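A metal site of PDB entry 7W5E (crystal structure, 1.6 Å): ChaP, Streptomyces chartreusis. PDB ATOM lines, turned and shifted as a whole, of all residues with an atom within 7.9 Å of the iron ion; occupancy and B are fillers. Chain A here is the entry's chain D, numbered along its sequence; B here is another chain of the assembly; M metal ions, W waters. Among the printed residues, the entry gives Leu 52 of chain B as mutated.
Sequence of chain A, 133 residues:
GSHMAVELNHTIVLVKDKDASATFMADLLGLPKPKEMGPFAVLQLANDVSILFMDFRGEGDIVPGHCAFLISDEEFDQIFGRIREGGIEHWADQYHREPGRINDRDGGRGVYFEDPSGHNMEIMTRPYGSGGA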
ATOM      1  N   PRO A  64      -4.742  25.460  36.428  1.00  0.00           N
ATOM      2  CA  PRO A  64      -4.646  24.917  35.064  1.00  0.00           C
ATOM      3  C   PRO A  64      -3.499  25.481  34.234  1.00  0.00           C
ATOM      4  O   PRO A  64      -3.589  25.417  33.005  1.00  0.00           O
ATOM      5  CB  PRO A  64      -5.985  25.306  34.453  1.00  0.00           C
ATOM      6  CG  PRO A  64      -6.335  26.590  35.118  1.00  0.00           C
ATOM      7  CD  PRO A  64      -5.724  26.561  36.500  1.00  0.00           C
ATOM      8  N   GLY A  65      -2.475  26.048  34.879  1.00  0.00           N
ATOM      9  CA  GLY A  65      -1.315  26.494  34.128  1.00  0.00           C
ATOM     10  C   GLY A  65      -0.649  25.353  33.382  1.00  0.00           C
ATOM     11  O   GLY A  65      -0.690  24.205  33.811  1.00  0.00           O
ATOM     12  N   HIS A  66      -0.066  25.687  32.238  1.00  0.00           N
ATOM     13  CA  HIS A  66       0.669  24.705  31.443  1.00  0.00           C
ATOM     14  C   HIS A  66       1.455  25.429  30.349  1.00  0.00           C
ATOM     15  O   HIS A  66       1.224  26.609  30.083  1.00  0.00           O
ATOM     16  CB  HIS A  66      -0.247  23.649  30.820  1.00  0.00           C
ATOM     17  CG  HIS A  66      -1.381  24.213  30.006  1.00  0.00           C
ATOM     18  ND1 HIS A  66      -2.494  24.796  30.571  1.00  0.00           N
ATOM     19  CD2 HIS A  66      -1.568  24.268  28.662  1.00  0.00           C
ATOM     20  CE1 HIS A  66      -3.323  25.174  29.606  1.00  0.00           C
ATOM     21  NE2 HIS A  66      -2.782  24.862  28.443  1.00  0.00           N
ATOM     22  N   CYS A  67       2.383  24.700  29.750  1.00  0.00           N
ATOM     23  CA  CYS A  67       3.025  25.081  28.496  1.00  0.00           C
ATOM     24  C   CYS A  67       2.564  24.128  27.406  1.00  0.00           C
ATOM     25  O   CYS A  67       2.625  22.900  27.584  1.00  0.00           O
ATOM     26  CB  CYS A  67       4.546  25.039  28.604  1.00  0.00           C
ATOM     27  SG  CYS A  67       5.300  26.298  29.646  1.00  0.00           S
ATOM     28  N   ALA A  68       2.121  24.665  26.274  1.00  0.00           N
ATOM     29  CA  ALA A  68       1.487  23.876  25.228  1.00  0.00           C
ATOM     30  C   ALA A  68       2.282  23.956  23.941  1.00  0.00           C
ATOM     31  O   ALA A  68       2.737  25.026  23.530  1.00  0.00           O
ATOM     32  CB  ALA A  68       0.073  24.344  24.975  1.00  0.00           C
ATOM     33  N   PHE A  69       2.439  22.793  23.297  1.00  0.00           N
ATOM     34  CA  PHE A  69       3.204  22.657  22.069  1.00  0.00           C
ATOM     35  C   PHE A  69       2.281  22.213  20.945  1.00  0.00           C
ATOM     36  O   PHE A  69       1.495  21.279  21.110  1.00  0.00           O
ATOM     37  CB  PHE A  69       4.365  21.681  22.257  1.00  0.00           C
ATOM     38  CG  PHE A  69       5.289  22.061  23.383  1.00  0.00           C
ATOM     39  CD1 PHE A  69       5.019  21.656  24.666  1.00  0.00           C
ATOM     40  CD2 PHE A  69       6.383  22.881  23.139  1.00  0.00           C
ATOM     41  CE1 PHE A  69       5.848  22.029  25.711  1.00  0.00           C
ATOM     42  CE2 PHE A  69       7.211  23.264  24.180  1.00  0.00           C
ATOM     43  CZ  PHE A  69       6.945  22.836  25.462  1.00  0.00           C
ATOM     44  N   GLN A  94      -7.018  20.613  31.048  1.00  0.00           N
ATOM     45  CA  GLN A  94      -5.999  21.409  31.730  1.00  0.00           C
ATOM     46  C   GLN A  94      -6.122  21.345  33.252  1.00  0.00           C
ATOM     47  O   GLN A  94      -5.174  21.734  33.951  1.00  0.00           O
ATOM     48  CB  GLN A  94      -6.079  22.860  31.243  1.00  0.00           C
ATOM     49  CG  GLN A  94      -7.436  23.499  31.474  1.00  0.00           C
ATOM     50  CD  GLN A  94      -7.501  24.914  30.950  1.00  0.00           C
ATOM     51  OE1 GLN A  94      -6.492  25.466  30.503  1.00  0.00           O
ATOM     52  NE2 GLN A  94      -8.687  25.507  30.971  1.00  0.00           N
ATOM     53  N   TYR A 112      -2.874  16.483  28.016  1.00  0.00           N
ATOM     54  CA  TYR A 112      -2.087  17.144  29.033  1.00  0.00           C
ATOM     55  C   TYR A 112      -1.335  16.106  29.864  1.00  0.00           C
ATOM     56  O   TYR A 112      -1.791  14.966  30.013  1.00  0.00           O
ATOM     57  CB  TYR A 112      -2.966  17.996  29.966  1.00  0.00           C
ATOM     58  CG  TYR A 112      -3.783  19.057  29.262  1.00  0.00           C
ATOM     59  CD1 TYR A 112      -4.949  18.718  28.570  1.00  0.00           C
ATOM     60  CD2 TYR A 112      -3.399  20.378  29.291  1.00  0.00           C
ATOM     61  CE1 TYR A 112      -5.703  19.690  27.928  1.00  0.00           C
ATOM     62  CE2 TYR A 112      -4.131  21.359  28.641  1.00  0.00           C
ATOM     63  CZ  TYR A 112      -5.289  21.006  27.967  1.00  0.00           C
ATOM     64  OH  TYR A 112      -6.026  21.984  27.339  1.00  0.00           O
ATOM     65  N   MET A 121       2.277  20.211  31.091  1.00  0.00           N
ATOM     66  CA  MET A 121       2.473  20.346  29.653  1.00  0.00           C
ATOM     67  C   MET A 121       1.179  20.023  28.917  1.00  0.00           C
ATOM     68  O   MET A 121       0.235  19.449  29.457  1.00  0.00           O
ATOM     69  CB  MET A 121       3.595  19.425  29.158  1.00  0.00           C
ATOM     70  CG  MET A 121       4.875  19.523  29.983  1.00  0.00           C
ATOM     71  SD  MET A 121       5.708  21.114  29.812  1.00  0.00           S
ATOM     72  CE  MET A 121       7.297  20.730  30.551  1.00  0.00           C
ATOM     73  N   GLU A 122       1.165  20.394  27.629  1.00  0.00           N
ATOM     74  CA  GLU A 122       0.092  20.060  26.708  1.00  0.00           C
ATOM     75  C   GLU A 122       0.712  19.867  25.337  1.00  0.00           C
ATOM     76  O   GLU A 122       1.627  20.608  24.982  1.00  0.00           O
ATOM     77  CB  GLU A 122      -0.983  21.155  26.645  1.00  0.00           C
ATOM     78  CG  GLU A 122      -2.175  20.829  25.742  1.00  0.00           C
ATOM     79  CD  GLU A 122      -3.060  22.040  25.494  1.00  0.00           C
ATOM     80  OE1 GLU A 122      -2.804  23.097  26.088  1.00  0.00           O
ATOM     81  OE2 GLU A 122      -4.031  21.915  24.703  1.00  0.00           O
ATOM     82  N   ILE A 123       0.252  18.866  24.596  1.00  0.00           N
ATOM     83  CA  ILE A 123       0.527  18.764  23.168  1.00  0.00           C
ATOM     84  C   ILE A 123      -0.807  18.794  22.435  1.00  0.00           C
ATOM     85  O   ILE A 123      -1.807  18.259  22.923  1.00  0.00           O
ATOM     86  CB  ILE A 123       1.333  17.503  22.804  1.00  0.00           C
ATOM     87  CG1 ILE A 123       0.645  16.234  23.331  1.00  0.00           C
ATOM     88  CG2 ILE A 123       2.752  17.616  23.333  1.00  0.00           C
ATOM     89  CD1 ILE A 123       1.280  14.939  22.830  1.00  0.00           C
ATOM     90  N   MET A 124      -0.822  19.438  21.269  1.00  0.00           N
ATOM     91  CA  MET A 124      -2.052  19.676  20.524  1.00  0.00           C
ATOM     92  C   MET A 124      -1.716  19.654  19.041  1.00  0.00           C
ATOM     93  O   MET A 124      -0.578  19.924  18.646  1.00  0.00           O
ATOM     94  CB  MET A 124      -2.688  21.027  20.893  1.00  0.00           C
ATOM     95  CG  MET A 124      -1.750  22.201  20.707  1.00  0.00           C
ATOM     96  SD  MET A 124      -2.389  23.763  21.341  1.00  0.00           S
ATOM     97  CE  MET A 124      -3.131  24.446  19.870  1.00  0.00           C
ATOM     98  N   ASN B   9       3.083  26.807  21.370  1.00  0.00           N
ATOM     99  CA  ASN B   9       1.850  27.473  20.953  1.00  0.00           C
ATOM    100  C   ASN B   9       1.310  28.439  22.000  1.00  0.00           C
ATOM    101  O   ASN B   9       0.798  29.505  21.637  1.00  0.00           O
ATOM    102  CB  ASN B   9       0.793  26.431  20.615  1.00  0.00           C
ATOM    103  CG  ASN B   9      -0.473  27.052  20.062  1.00  0.00           C
ATOM    104  OD1 ASN B   9      -1.423  27.296  20.799  1.00  0.00           O
ATOM    105  ND2 ASN B   9      -0.486  27.310  18.761  1.00  0.00           N
ATOM    106  N   HIS B  10       1.364  28.081  23.283  1.00  0.00           N
ATOM    107  CA  HIS B  10       0.966  29.038  24.308  1.00  0.00           C
ATOM    108  C   HIS B  10       1.519  28.594  25.658  1.00  0.00           C
ATOM    109  O   HIS B  10       1.929  27.450  25.842  1.00  0.00           O
ATOM    110  CB  HIS B  10      -0.559  29.234  24.375  1.00  0.00           C
ATOM    111  CG  HIS B  10      -1.347  27.980  24.601  1.00  0.00           C
ATOM    112  ND1 HIS B  10      -1.706  27.127  23.582  1.00  0.00           N
ATOM    113  CD2 HIS B  10      -1.900  27.475  25.739  1.00  0.00           C
ATOM    114  CE1 HIS B  10      -2.423  26.133  24.077  1.00  0.00           C
ATOM    115  NE2 HIS B  10      -2.559  26.326  25.379  1.00  0.00           N
ATOM    116  N   THR B  11       1.579  29.560  26.582  1.00  0.00           N
ATOM    117  CA  THR B  11       2.004  29.296  27.951  1.00  0.00           C
ATOM    118  C   THR B  11       1.202  30.185  28.882  1.00  0.00           C
ATOM    119  O   THR B  11       0.825  31.299  28.531  1.00  0.00           O
ATOM    120  CB  THR B  11       3.510  29.525  28.154  1.00  0.00           C
ATOM    121  OG1 THR B  11       3.874  29.121  29.479  1.00  0.00           O
ATOM    122  CG2 THR B  11       3.879  30.995  27.958  1.00  0.00           C
ATOM    123  N   ILE B  12       0.905  29.642  30.064  1.00  0.00           N
ATOM    124  CA  ILE B  12       0.109  30.325  31.073  1.00  0.00           C
ATOM    125  C   ILE B  12       1.059  30.996  32.055  1.00  0.00           C
ATOM    126  O   ILE B  12       1.997  30.368  32.548  1.00  0.00           O
ATOM    127  CB  ILE B  12      -0.839  29.346  31.792  1.00  0.00           C
ATOM    128  CG1 ILE B  12      -2.075  29.026  30.940  1.00  0.00           C
ATOM    129  CG2 ILE B  12      -1.312  29.929  33.141  1.00  0.00           C
ATOM    130  CD1 ILE B  12      -1.805  28.326  29.607  1.00  0.00           C
ATOM    131  N   PHE B  40      -8.465  32.942  31.879  1.00  0.00           N
ATOM    132  CA  PHE B  40      -7.284  33.589  31.338  1.00  0.00           C
ATOM    133  C   PHE B  40      -7.608  34.889  30.625  1.00  0.00           C
ATOM    134  O   PHE B  40      -8.703  35.080  30.091  1.00  0.00           O
ATOM    135  CB  PHE B  40      -6.556  32.653  30.358  1.00  0.00           C
ATOM    136  CG  PHE B  40      -6.234  31.309  30.931  1.00  0.00           C
ATOM    137  CD1 PHE B  40      -5.413  31.195  32.052  1.00  0.00           C
ATOM    138  CD2 PHE B  40      -6.723  30.148  30.339  1.00  0.00           C
ATOM    139  CE1 PHE B  40      -5.108  29.952  32.584  1.00  0.00           C
ATOM    140  CE2 PHE B  40      -6.406  28.903  30.864  1.00  0.00           C
ATOM    141  CZ  PHE B  40      -5.598  28.801  31.988  1.00  0.00           C
ATOM    142  N   LEU B  52      -1.090  33.462  28.175  1.00  0.00           N
ATOM    143  CA  LEU B  52      -2.364  33.387  28.878  1.00  0.00           C
ATOM    144  C   LEU B  52      -2.143  33.776  30.335  1.00  0.00           C
ATOM    145  O   LEU B  52      -1.599  32.986  31.125  1.00  0.00           O
ATOM    146  CB  LEU B  52      -2.961  31.980  28.753  1.00  0.00           C
ATOM    147  CG  LEU B  52      -3.721  31.673  27.450  1.00  0.00           C
ATOM    148  CD1 LEU B  52      -2.779  31.544  26.260  1.00  0.00           C
ATOM    149  CD2 LEU B  52      -4.532  30.402  27.610  1.00  0.00           C
HETATM  150 FE    FE M   1      -3.639  24.892  26.503  1.00  0.00          FE
HETATM  151  O   HOH W   1      -4.991  24.192  24.585  1.00  0.00           O
HETATM  152  O   HOH W   2      -5.235  26.567  27.014  1.00  0.00           O
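OE1 of Glu 122 is bound to the iron ion, at 2.0 Å. NE2 of His 10 of chain B is bound to the iron ion, at 2.1 Å. The iron ion is bound by a ring nitrogen (NE2) of His 66, at 2.1 Å. The iron ion is bound by water W2. Water W1 binds the iron ion.
Merely in contact with the iron ion: Tyr 112 (3.9 Å). Of the 18 residues printed, 4 come within 4 Å of the iron ion.
O of Cys 67 lies within hydrogen-bond range of N of Glu 122 (2.9 Å). The backbone NH (N) of Phe 69 lies within hydrogen-bond range of the backbone carbonyl oxygen (O) of Glu 122. O of His 10 of chain B is in hydrogen-bond range of N of Ala 68. The backbone carbonyl oxygen of Pro 64 sits at hydrogen-bond distance from a ring nitrogen (ND1) of His 66 (2.7 Å). The side-chain carboxylate (OE2) of Glu 122 sits at hydrogen-bond distance from the side-chain hydroxyl (OH) of Tyr 112 (3.3 Å). The backbone carbonyl oxygen (O) of His 66 lies within hydrogen-bond range of the backbone NH (N) of Ile 12 of chain B, at 3.0 Å. The side-chain amide oxygen of Asn 9 of chain B lies within hydrogen-bond range of a ring nitrogen (ND1) of His 10 of chain B (2.8 Å).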
